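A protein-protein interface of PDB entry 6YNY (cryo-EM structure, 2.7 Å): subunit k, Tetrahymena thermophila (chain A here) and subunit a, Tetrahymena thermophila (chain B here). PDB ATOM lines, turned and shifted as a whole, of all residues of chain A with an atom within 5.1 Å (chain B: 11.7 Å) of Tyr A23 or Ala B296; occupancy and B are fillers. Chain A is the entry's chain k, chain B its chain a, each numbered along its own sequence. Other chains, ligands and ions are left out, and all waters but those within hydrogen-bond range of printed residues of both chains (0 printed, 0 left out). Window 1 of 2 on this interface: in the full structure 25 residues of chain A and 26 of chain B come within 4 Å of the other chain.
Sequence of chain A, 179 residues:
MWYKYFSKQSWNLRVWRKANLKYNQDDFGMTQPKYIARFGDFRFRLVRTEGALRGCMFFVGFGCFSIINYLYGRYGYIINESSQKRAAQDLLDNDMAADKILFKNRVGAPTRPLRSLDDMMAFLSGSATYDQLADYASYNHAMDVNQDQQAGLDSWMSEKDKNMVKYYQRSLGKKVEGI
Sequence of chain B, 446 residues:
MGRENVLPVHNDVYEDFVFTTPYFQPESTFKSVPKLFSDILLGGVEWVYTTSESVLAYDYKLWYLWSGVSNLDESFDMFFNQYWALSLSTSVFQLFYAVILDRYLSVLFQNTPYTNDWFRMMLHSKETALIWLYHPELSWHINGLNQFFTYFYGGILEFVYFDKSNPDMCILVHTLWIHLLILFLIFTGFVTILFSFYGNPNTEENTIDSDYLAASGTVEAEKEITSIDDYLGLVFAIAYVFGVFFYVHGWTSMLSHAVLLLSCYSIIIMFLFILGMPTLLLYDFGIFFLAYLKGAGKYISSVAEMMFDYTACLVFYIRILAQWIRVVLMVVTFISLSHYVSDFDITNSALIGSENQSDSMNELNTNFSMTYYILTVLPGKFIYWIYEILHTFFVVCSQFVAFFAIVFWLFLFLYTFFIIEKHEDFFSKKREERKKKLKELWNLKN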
ATOM      1  N   ASN A  20     -13.681   7.275  -4.563  1.00  0.00           N
ATOM      2  CA  ASN A  20     -13.967   6.548  -3.337  1.00  0.00           C
ATOM      3  C   ASN A  20     -15.210   5.694  -3.544  1.00  0.00           C
ATOM      4  O   ASN A  20     -16.275   6.213  -3.895  1.00  0.00           O
ATOM      5  CB  ASN A  20     -14.167   7.507  -2.168  1.00  0.00           C
ATOM      6  CG  ASN A  20     -14.627   6.807  -0.920  1.00  0.00           C
ATOM      7  OD1 ASN A  20     -14.305   5.643  -0.690  1.00  0.00           O
ATOM      8  ND2 ASN A  20     -15.392   7.509  -0.106  1.00  0.00           N
ATOM      9  N   LEU A  21     -15.072   4.390  -3.327  1.00  0.00           N
ATOM     10  CA  LEU A  21     -16.185   3.476  -3.521  1.00  0.00           C
ATOM     11  C   LEU A  21     -17.191   3.529  -2.384  1.00  0.00           C
ATOM     12  O   LEU A  21     -18.336   3.108  -2.571  1.00  0.00           O
ATOM     13  CB  LEU A  21     -15.668   2.050  -3.679  1.00  0.00           C
ATOM     14  CG  LEU A  21     -14.570   1.875  -4.722  1.00  0.00           C
ATOM     15  CD1 LEU A  21     -14.225   0.423  -4.863  1.00  0.00           C
ATOM     16  CD2 LEU A  21     -14.989   2.451  -6.048  1.00  0.00           C
ATOM     17  N   LYS A  22     -16.796   4.027  -1.217  1.00  0.00           N
ATOM     18  CA  LYS A  22     -17.714   4.160  -0.090  1.00  0.00           C
ATOM     19  C   LYS A  22     -18.457   5.489  -0.140  1.00  0.00           C
ATOM     20  O   LYS A  22     -18.543   6.203   0.853  1.00  0.00           O
ATOM     21  CB  LYS A  22     -16.952   4.031   1.221  1.00  0.00           C
ATOM     22  CG  LYS A  22     -16.113   2.795   1.371  1.00  0.00           C
ATOM     23  CD  LYS A  22     -15.419   2.801   2.720  1.00  0.00           C
ATOM     24  CE  LYS A  22     -14.517   1.604   2.899  1.00  0.00           C
ATOM     25  NZ  LYS A  22     -15.264   0.325   2.811  1.00  0.00           N
ATOM     26  N   TYR A  23     -19.029   5.817  -1.292  1.00  0.00           N
ATOM     27  CA  TYR A  23     -19.755   7.064  -1.481  1.00  0.00           C
ATOM     28  C   TYR A  23     -21.228   6.739  -1.659  1.00  0.00           C
ATOM     29  O   TYR A  23     -21.594   5.953  -2.540  1.00  0.00           O
ATOM     30  CB  TYR A  23     -19.219   7.840  -2.681  1.00  0.00           C
ATOM     31  CG  TYR A  23     -20.017   9.076  -3.007  1.00  0.00           C
ATOM     32  CD1 TYR A  23     -20.073  10.136  -2.121  1.00  0.00           C
ATOM     33  CD2 TYR A  23     -20.707   9.185  -4.201  1.00  0.00           C
ATOM     34  CE1 TYR A  23     -20.801  11.266  -2.411  1.00  0.00           C
ATOM     35  CE2 TYR A  23     -21.436  10.311  -4.500  1.00  0.00           C
ATOM     36  CZ  TYR A  23     -21.480  11.348  -3.600  1.00  0.00           C
ATOM     37  OH  TYR A  23     -22.204  12.475  -3.896  1.00  0.00           O
ATOM     38  N   ASN A  24     -22.070   7.349  -0.827  1.00  0.00           N
ATOM     39  CA  ASN A  24     -23.506   7.094  -0.851  1.00  0.00           C
ATOM     40  C   ASN A  24     -24.113   7.840  -2.033  1.00  0.00           C
ATOM     41  O   ASN A  24     -24.715   8.908  -1.904  1.00  0.00           O
ATOM     42  CB  ASN A  24     -24.145   7.498   0.467  1.00  0.00           C
ATOM     43  CG  ASN A  24     -25.536   6.936   0.631  1.00  0.00           C
ATOM     44  OD1 ASN A  24     -26.040   6.229  -0.239  1.00  0.00           O
ATOM     45  ND2 ASN A  24     -26.158   7.232   1.760  1.00  0.00           N
ATOM     46  N   GLN A  25     -23.940   7.253  -3.215  1.00  0.00           N
ATOM     47  CA  GLN A  25     -24.540   7.797  -4.421  1.00  0.00           C
ATOM     48  C   GLN A  25     -26.039   7.550  -4.487  1.00  0.00           C
ATOM     49  O   GLN A  25     -26.708   8.133  -5.345  1.00  0.00           O
ATOM     50  CB  GLN A  25     -23.861   7.205  -5.654  1.00  0.00           C
ATOM     51  CG  GLN A  25     -23.901   5.696  -5.729  1.00  0.00           C
ATOM     52  CD  GLN A  25     -23.417   5.151  -7.060  1.00  0.00           C
ATOM     53  OE1 GLN A  25     -23.743   4.025  -7.431  1.00  0.00           O
ATOM     54  NE2 GLN A  25     -22.636   5.942  -7.782  1.00  0.00           N
ATOM     55  N   PHE A  28     -27.230  10.883  -2.298  1.00  0.00           N
ATOM     56  CA  PHE A  28     -26.743  12.194  -2.692  1.00  0.00           C
ATOM     57  C   PHE A  28     -26.398  12.186  -4.170  1.00  0.00           C
ATOM     58  O   PHE A  28     -25.844  11.210  -4.680  1.00  0.00           O
ATOM     59  CB  PHE A  28     -25.504  12.611  -1.894  1.00  0.00           C
ATOM     60  CG  PHE A  28     -25.636  12.421  -0.418  1.00  0.00           C
ATOM     61  CD1 PHE A  28     -24.792  11.563   0.256  1.00  0.00           C
ATOM     62  CD2 PHE A  28     -26.603  13.097   0.296  1.00  0.00           C
ATOM     63  CE1 PHE A  28     -24.907  11.386   1.613  1.00  0.00           C
ATOM     64  CE2 PHE A  28     -26.722  12.922   1.653  1.00  0.00           C
ATOM     65  CZ  PHE A  28     -25.875  12.065   2.312  1.00  0.00           C
ATOM     66  N   GLY A  29     -26.726  13.276  -4.846  1.00  0.00           N
ATOM     67  CA  GLY A  29     -26.302  13.482  -6.212  1.00  0.00           C
ATOM     68  C   GLY A  29     -27.370  13.155  -7.231  1.00  0.00           C
ATOM     69  O   GLY A  29     -28.529  12.867  -6.922  1.00  0.00           O
ATOM     70  N   GLU A  50     -21.441  10.299 -11.270  1.00  0.00           N
ATOM     71  CA  GLU A  50     -21.822  11.582 -11.846  1.00  0.00           C
ATOM     72  C   GLU A  50     -20.616  12.480 -12.076  1.00  0.00           C
ATOM     73  O   GLU A  50     -20.616  13.280 -13.018  1.00  0.00           O
ATOM     74  CB  GLU A  50     -22.828  12.289 -10.938  1.00  0.00           C
ATOM     75  CG  GLU A  50     -22.294  12.647  -9.571  1.00  0.00           C
ATOM     76  CD  GLU A  50     -23.308  13.381  -8.727  1.00  0.00           C
ATOM     77  OE1 GLU A  50     -24.445  13.573  -9.199  1.00  0.00           O
ATOM     78  OE2 GLU A  50     -22.968  13.771  -7.592  1.00  0.00           O
ATOM     79  N   ARG A  54     -20.346  14.270 -15.641  1.00  0.00           N
ATOM     80  CA  ARG A  54     -20.310  15.722 -15.751  1.00  0.00           C
ATOM     81  C   ARG A  54     -19.012  16.202 -16.380  1.00  0.00           C
ATOM     82  O   ARG A  54     -19.001  17.219 -17.080  1.00  0.00           O
ATOM     83  CB  ARG A  54     -20.496  16.355 -14.375  1.00  0.00           C
ATOM     84  CG  ARG A  54     -21.881  16.184 -13.796  1.00  0.00           C
ATOM     85  CD  ARG A  54     -22.059  17.030 -12.556  1.00  0.00           C
ATOM     86  NE  ARG A  54     -21.409  16.450 -11.389  1.00  0.00           N
ATOM     87  CZ  ARG A  54     -21.126  17.122 -10.281  1.00  0.00           C
ATOM     88  NH1 ARG A  54     -21.423  18.407 -10.184  1.00  0.00           N
ATOM     89  NH2 ARG A  54     -20.540  16.509  -9.267  1.00  0.00           N
ATOM     90  N   PHE B 288     -13.048  14.343 -12.698  1.00  0.00           N
ATOM     91  CA  PHE B 288     -13.963  14.701 -11.625  1.00  0.00           C
ATOM     92  C   PHE B 288     -13.843  16.155 -11.199  1.00  0.00           C
ATOM     93  O   PHE B 288     -14.431  16.533 -10.182  1.00  0.00           O
ATOM     94  CB  PHE B 288     -13.715  13.812 -10.406  1.00  0.00           C
ATOM     95  CG  PHE B 288     -14.117  12.385 -10.597  1.00  0.00           C
ATOM     96  CD1 PHE B 288     -15.203  11.867  -9.921  1.00  0.00           C
ATOM     97  CD2 PHE B 288     -13.407  11.560 -11.443  1.00  0.00           C
ATOM     98  CE1 PHE B 288     -15.572  10.557 -10.090  1.00  0.00           C
ATOM     99  CE2 PHE B 288     -13.775  10.249 -11.614  1.00  0.00           C
ATOM    100  CZ  PHE B 288     -14.858   9.748 -10.939  1.00  0.00           C
ATOM    101  N   PHE B 289     -13.112  16.977 -11.954  1.00  0.00           N
ATOM    102  CA  PHE B 289     -12.798  18.325 -11.496  1.00  0.00           C
ATOM    103  C   PHE B 289     -14.046  19.119 -11.143  1.00  0.00           C
ATOM    104  O   PHE B 289     -13.988  20.014 -10.294  1.00  0.00           O
ATOM    105  CB  PHE B 289     -11.983  19.054 -12.561  1.00  0.00           C
ATOM    106  CG  PHE B 289     -12.737  19.336 -13.824  1.00  0.00           C
ATOM    107  CD1 PHE B 289     -12.973  18.332 -14.740  1.00  0.00           C
ATOM    108  CD2 PHE B 289     -13.187  20.609 -14.108  1.00  0.00           C
ATOM    109  CE1 PHE B 289     -13.657  18.588 -15.903  1.00  0.00           C
ATOM    110  CE2 PHE B 289     -13.871  20.868 -15.271  1.00  0.00           C
ATOM    111  CZ  PHE B 289     -14.105  19.855 -16.168  1.00  0.00           C
ATOM    112  N   LEU B 290     -15.182  18.806 -11.763  1.00  0.00           N
ATOM    113  CA  LEU B 290     -16.394  19.566 -11.490  1.00  0.00           C
ATOM    114  C   LEU B 290     -16.966  19.249 -10.116  1.00  0.00           C
ATOM    115  O   LEU B 290     -17.571  20.121  -9.484  1.00  0.00           O
ATOM    116  CB  LEU B 290     -17.429  19.294 -12.573  1.00  0.00           C
ATOM    117  CG  LEU B 290     -17.100  19.888 -13.937  1.00  0.00           C
ATOM    118  CD1 LEU B 290     -18.078  19.403 -14.971  1.00  0.00           C
ATOM    119  CD2 LEU B 290     -17.106  21.399 -13.870  1.00  0.00           C
ATOM    120  N   ALA B 291     -16.789  18.019  -9.639  1.00  0.00           N
ATOM    121  CA  ALA B 291     -17.223  17.686  -8.289  1.00  0.00           C
ATOM    122  C   ALA B 291     -16.348  18.352  -7.239  1.00  0.00           C
ATOM    123  O   ALA B 291     -16.819  18.643  -6.135  1.00  0.00           O
ATOM    124  CB  ALA B 291     -17.219  16.173  -8.099  1.00  0.00           C
ATOM    125  N   TYR B 292     -15.078  18.601  -7.560  1.00  0.00           N
ATOM    126  CA  TYR B 292     -14.208  19.303  -6.628  1.00  0.00           C
ATOM    127  C   TYR B 292     -14.653  20.744  -6.427  1.00  0.00           C
ATOM    128  O   TYR B 292     -14.378  21.336  -5.378  1.00  0.00           O
ATOM    129  CB  TYR B 292     -12.767  19.265  -7.129  1.00  0.00           C
ATOM    130  CG  TYR B 292     -12.107  17.909  -7.059  1.00  0.00           C
ATOM    131  CD1 TYR B 292     -12.360  16.941  -8.014  1.00  0.00           C
ATOM    132  CD2 TYR B 292     -11.217  17.605  -6.046  1.00  0.00           C
ATOM    133  CE1 TYR B 292     -11.756  15.708  -7.953  1.00  0.00           C
ATOM    134  CE2 TYR B 292     -10.609  16.376  -5.979  1.00  0.00           C
ATOM    135  CZ  TYR B 292     -10.879  15.431  -6.933  1.00  0.00           C
ATOM    136  OH  TYR B 292     -10.268  14.202  -6.862  1.00  0.00           O
ATOM    137  N   LEU B 293     -15.333  21.324  -7.414  1.00  0.00           N
ATOM    138  CA  LEU B 293     -15.759  22.717  -7.343  1.00  0.00           C
ATOM    139  C   LEU B 293     -17.163  22.855  -6.763  1.00  0.00           C
ATOM    140  O   LEU B 293     -17.355  23.502  -5.729  1.00  0.00           O
ATOM    141  CB  LEU B 293     -15.715  23.346  -8.738  1.00  0.00           C
ATOM    142  CG  LEU B 293     -14.420  23.195  -9.524  1.00  0.00           C
ATOM    143  CD1 LEU B 293     -14.608  23.743 -10.912  1.00  0.00           C
ATOM    144  CD2 LEU B 293     -13.292  23.901  -8.831  1.00  0.00           C
ATOM    145  N   LYS B 294     -18.147  22.248  -7.419  1.00  0.00           N
ATOM    146  CA  LYS B 294     -19.546  22.428  -7.054  1.00  0.00           C
ATOM    147  C   LYS B 294     -20.061  21.342  -6.124  1.00  0.00           C
ATOM    148  O   LYS B 294     -20.975  21.600  -5.334  1.00  0.00           O
ATOM    149  CB  LYS B 294     -20.411  22.460  -8.315  1.00  0.00           C
ATOM    150  CG  LYS B 294     -21.855  22.850  -8.066  1.00  0.00           C
ATOM    151  CD  LYS B 294     -22.684  22.767  -9.332  1.00  0.00           C
ATOM    152  CE  LYS B 294     -22.974  21.328  -9.706  1.00  0.00           C
ATOM    153  NZ  LYS B 294     -23.831  21.214 -10.918  1.00  0.00           N
ATOM    154  N   GLY B 295     -19.502  20.141  -6.200  1.00  0.00           N
ATOM    155  CA  GLY B 295     -19.978  19.039  -5.393  1.00  0.00           C
ATOM    156  C   GLY B 295     -20.903  18.123  -6.162  1.00  0.00           C
ATOM    157  O   GLY B 295     -20.780  17.984  -7.382  1.00  0.00           O
ATOM    158  N   ALA B 296     -21.840  17.497  -5.460  1.00  0.00           N
ATOM    159  CA  ALA B 296     -22.769  16.572  -6.088  1.00  0.00           C
ATOM    160  C   ALA B 296     -23.925  17.325  -6.729  1.00  0.00           C
ATOM    161  O   ALA B 296     -24.382  18.350  -6.215  1.00  0.00           O
ATOM    162  CB  ALA B 296     -23.304  15.573  -5.066  1.00  0.00           C
ATOM    163  N   GLY B 297     -24.391  16.810  -7.859  1.00  0.00           N
ATOM    164  CA  GLY B 297     -25.493  17.415  -8.568  1.00  0.00           C
ATOM    165  C   GLY B 297     -26.800  17.274  -7.815  1.00  0.00           C
ATOM    166  O   GLY B 297     -26.881  16.716  -6.720  1.00  0.00           O
ATOM    167  N   LYS B 298     -27.854  17.800  -8.432  1.00  0.00           N
ATOM    168  CA  LYS B 298     -29.180  17.770  -7.832  1.00  0.00           C
ATOM    169  C   LYS B 298     -30.217  17.163  -8.768  1.00  0.00           C
ATOM    170  O   LYS B 298     -31.141  16.482  -8.316  1.00  0.00           O
ATOM    171  CB  LYS B 298     -29.602  19.183  -7.430  1.00  0.00           C
ATOM    172  CG  LYS B 298     -30.842  19.230  -6.567  1.00  0.00           C
ATOM    173  CD  LYS B 298     -31.177  20.648  -6.158  1.00  0.00           C
ATOM    174  CE  LYS B 298     -32.353  20.679  -5.198  1.00  0.00           C
ATOM    175  NZ  LYS B 298     -33.569  20.041  -5.773  1.00  0.00           N
ATOM    176  N   TYR B 299     -30.072  17.395 -10.069  1.00  0.00           N
ATOM    177  CA  TYR B 299     -31.048  16.955 -11.051  1.00  0.00           C
ATOM    178  C   TYR B 299     -30.481  15.839 -11.919  1.00  0.00           C
ATOM    179  O   TYR B 299     -29.281  15.789 -12.196  1.00  0.00           O
ATOM    180  CB  TYR B 299     -31.478  18.119 -11.945  1.00  0.00           C
ATOM    181  CG  TYR B 299     -31.858  19.364 -11.184  1.00  0.00           C
ATOM    182  CD1 TYR B 299     -31.008  20.457 -11.142  1.00  0.00           C
ATOM    183  CD2 TYR B 299     -33.058  19.443 -10.499  1.00  0.00           C
ATOM    184  CE1 TYR B 299     -31.346  21.595 -10.447  1.00  0.00           C
ATOM    185  CE2 TYR B 299     -33.404  20.577  -9.801  1.00  0.00           C
ATOM    186  CZ  TYR B 299     -32.545  21.650  -9.777  1.00  0.00           C
ATOM    187  OH  TYR B 299     -32.891  22.781  -9.078  1.00  0.00           O
ATOM    188  N   ILE B 300     -31.374  14.947 -12.355  1.00  0.00           N
ATOM    189  CA  ILE B 300     -30.978  13.831 -13.202  1.00  0.00           C
ATOM    190  C   ILE B 300     -30.607  14.276 -14.606  1.00  0.00           C
ATOM    191  O   ILE B 300     -29.995  13.505 -15.353  1.00  0.00           O
ATOM    192  CB  ILE B 300     -32.105  12.785 -13.265  1.00  0.00           C
ATOM    193  CG1 ILE B 300     -33.369  13.398 -13.867  1.00  0.00           C
ATOM    194  CG2 ILE B 300     -32.399  12.247 -11.887  1.00  0.00           C
ATOM    195  CD1 ILE B 300     -34.522  12.449 -13.934  1.00  0.00           C
ATOM    196  N   SER B 301     -30.963  15.496 -14.993  1.00  0.00           N
ATOM    197  CA  SER B 301     -30.691  15.976 -16.339  1.00  0.00           C
ATOM    198  C   SER B 301     -29.233  16.395 -16.457  1.00  0.00           C
ATOM    199  O   SER B 301     -28.774  17.281 -15.728  1.00  0.00           O
ATOM    200  CB  SER B 301     -31.611  17.142 -16.683  1.00  0.00           C
ATOM    201  OG  SER B 301     -31.350  17.621 -17.988  1.00  0.00           O
ATOM    202  N   SER B 302     -28.507  15.761 -17.376  1.00  0.00           N
ATOM    203  CA  SER B 302     -27.121  16.145 -17.605  1.00  0.00           C
ATOM    204  C   SER B 302     -27.028  17.510 -18.269  1.00  0.00           C
ATOM    205  O   SER B 302     -26.060  18.243 -18.042  1.00  0.00           O
ATOM    206  CB  SER B 302     -26.420  15.091 -18.457  1.00  0.00           C
ATOM    207  OG  SER B 302     -27.072  14.929 -19.701  1.00  0.00           O
ATOM    208  N   ALA B 304     -29.070  19.991 -17.663  1.00  0.00           N
ATOM    209  CA  ALA B 304     -29.296  20.964 -16.603  1.00  0.00           C
ATOM    210  C   ALA B 304     -28.024  21.192 -15.801  1.00  0.00           C
ATOM    211  O   ALA B 304     -27.573  22.331 -15.637  1.00  0.00           O
ATOM    212  CB  ALA B 304     -30.424  20.492 -15.691  1.00  0.00           C
ATOM    213  N   GLU B 305     -27.428  20.113 -15.293  1.00  0.00           N
ATOM    214  CA  GLU B 305     -26.186  20.248 -14.547  1.00  0.00           C
ATOM    215  C   GLU B 305     -25.085  20.842 -15.410  1.00  0.00           C
ATOM    216  O   GLU B 305     -24.236  21.585 -14.907  1.00  0.00           O
ATOM    217  CB  GLU B 305     -25.756  18.891 -14.000  1.00  0.00           C
ATOM    218  CG  GLU B 305     -26.763  18.264 -13.056  1.00  0.00           C
ATOM    219  CD  GLU B 305     -27.001  19.097 -11.814  1.00  0.00           C
ATOM    220  OE1 GLU B 305     -26.199  20.017 -11.548  1.00  0.00           O
ATOM    221  OE2 GLU B 305     -27.993  18.836 -11.104  1.00  0.00           O
ATOM    222  N   MET B 306     -25.088  20.538 -16.709  1.00  0.00           N
ATOM    223  CA  MET B 306     -24.077  21.093 -17.598  1.00  0.00           C
ATOM    224  C   MET B 306     -24.011  22.607 -17.482  1.00  0.00           C
ATOM    225  O   MET B 306     -22.929  23.193 -17.588  1.00  0.00           O
ATOM    226  CB  MET B 306     -24.376  20.689 -19.042  1.00  0.00           C
ATOM    227  CG  MET B 306     -23.312  21.102 -20.035  1.00  0.00           C
ATOM    228  SD  MET B 306     -23.843  20.944 -21.749  1.00  0.00           S
ATOM    229  CE  MET B 306     -24.113  19.181 -21.855  1.00  0.00           C
ATOM    230  N   PHE B 308     -25.061  24.445 -14.707  1.00  0.00           N
ATOM    231  CA  PHE B 308     -24.577  24.773 -13.375  1.00  0.00           C
ATOM    232  C   PHE B 308     -23.095  24.473 -13.221  1.00  0.00           C
ATOM    233  O   PHE B 308     -22.438  25.079 -12.368  1.00  0.00           O
ATOM    234  CB  PHE B 308     -25.380  24.007 -12.328  1.00  0.00           C
ATOM    235  CG  PHE B 308     -26.782  24.505 -12.163  1.00  0.00           C
ATOM    236  CD1 PHE B 308     -27.120  25.327 -11.106  1.00  0.00           C
ATOM    237  CD2 PHE B 308     -27.762  24.160 -13.074  1.00  0.00           C
ATOM    238  CE1 PHE B 308     -28.409  25.790 -10.958  1.00  0.00           C
ATOM    239  CE2 PHE B 308     -29.051  24.620 -12.931  1.00  0.00           C
ATOM    240  CZ  PHE B 308     -29.375  25.435 -11.873  1.00  0.00           C
ATOM    241  N   ASP B 309     -22.558  23.558 -14.026  1.00  0.00           N
ATOM    242  CA  ASP B 309     -21.134  23.264 -13.971  1.00  0.00           C
ATOM    243  C   ASP B 309     -20.318  24.286 -14.747  1.00  0.00           C
ATOM    244  O   ASP B 309     -19.174  24.568 -14.378  1.00  0.00           O
ATOM    245  CB  ASP B 309     -20.871  21.858 -14.505  1.00  0.00           C
ATOM    246  CG  ASP B 309     -21.321  20.777 -13.541  1.00  0.00           C
ATOM    247  OD1 ASP B 309     -22.537  20.514 -13.455  1.00  0.00           O
ATOM    248  OD2 ASP B 309     -20.458  20.189 -12.861  1.00  0.00           O
ATOM    249  N   THR B 311     -21.086  27.453 -14.839  1.00  0.00           N
ATOM    250  CA  THR B 311     -20.997  28.584 -13.924  1.00  0.00           C
ATOM    251  C   THR B 311     -19.884  28.372 -12.908  1.00  0.00           C
ATOM    252  O   THR B 311     -19.060  29.264 -12.675  1.00  0.00           O
ATOM    253  CB  THR B 311     -22.332  28.789 -13.211  1.00  0.00           C
ATOM    254  OG1 THR B 311     -22.684  27.597 -12.502  1.00  0.00           O
ATOM    255  CG2 THR B 311     -23.420  29.113 -14.208  1.00  0.00           C
ATOM    256  N   ALA B 312     -19.839  27.188 -12.298  1.00  0.00           N
ATOM    257  CA  ALA B 312     -18.810  26.908 -11.306  1.00  0.00           C
ATOM    258  C   ALA B 312     -17.417  27.018 -11.910  1.00  0.00           C
ATOM    259  O   ALA B 312     -16.481  27.482 -11.249  1.00  0.00           O
ATOM    260  CB  ALA B 312     -19.027  25.521 -10.709  1.00  0.00           C
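Among the printed residues, pairs that only touch across the chains: Tyr A23 with Ala B296 (3.5 Å), Gly A29 with Ala B296 (3.8 Å), Gly A29 with Gly B297 (3.3 Å), Glu A50 with Ala B296 (3.1 Å), Arg A54 with Leu B290 (3.2 Å), Arg A54 with Ala B291 (3.5 Å), Arg A54 with Lys B294 (3.3 Å) and Arg A54 with Ala B296 (3.9 Å).
Of chain B, only Ala B296 (3.5 Å) comes within 4 Å of Tyr A23.
No residue of chain B comes within 4 Å of Asn A20.
No residue of chain B comes within 4 Å of Gln A25.
No residue of chain B comes within 4 Å of Phe A28.
Gly A29 touches just these residues of chain B: Ala B296 (3.8 Å) and Gly B297 (3.3 Å).
Of the printed residues of chain A, Asp B309 touches Arg A54 (3.4 Å).
Of the printed residues of chain A, Ala B291 touches Arg A54.
Of the printed residues of chain B, Glu A50 touches Ala B296 and Gly B297.
The nearest residue of chain B that does not touch Tyr A23 is Gly B295 (6.2 Å).
The nearest printed residue of chain B that does not touch Arg A54 is Gly B297 (4.1 Å).
Of the 10 printed residues of chain A, 4 touch a printed residue of chain B.
Hydrophobic or aromatic side chains of chain A that line the printed part of chain B: Tyr A23.
OD2 of Asp B309 lies within salt-bridge range of NH1 of Arg A54 (3.4 Å).
The backbone carbonyl oxygen of Gly B295 lies within hydrogen-bond range of the guanidinium group of Arg A54.
OE2 of Glu A50 lies within hydrogen-bond range of N of Gly B297 (3.4 Å).
OE1 of Glu B305 is in salt-bridge range of NZ of Lys B294, at 2.7 Å.
O of Glu B305 lies close to OD1 of Asp B309 (2.5 Å).
The side-chain amino group (NZ) of Lys B294 lies within salt-bridge range of the side-chain carboxylate (OD1) of Asp B309 (2.9 Å).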
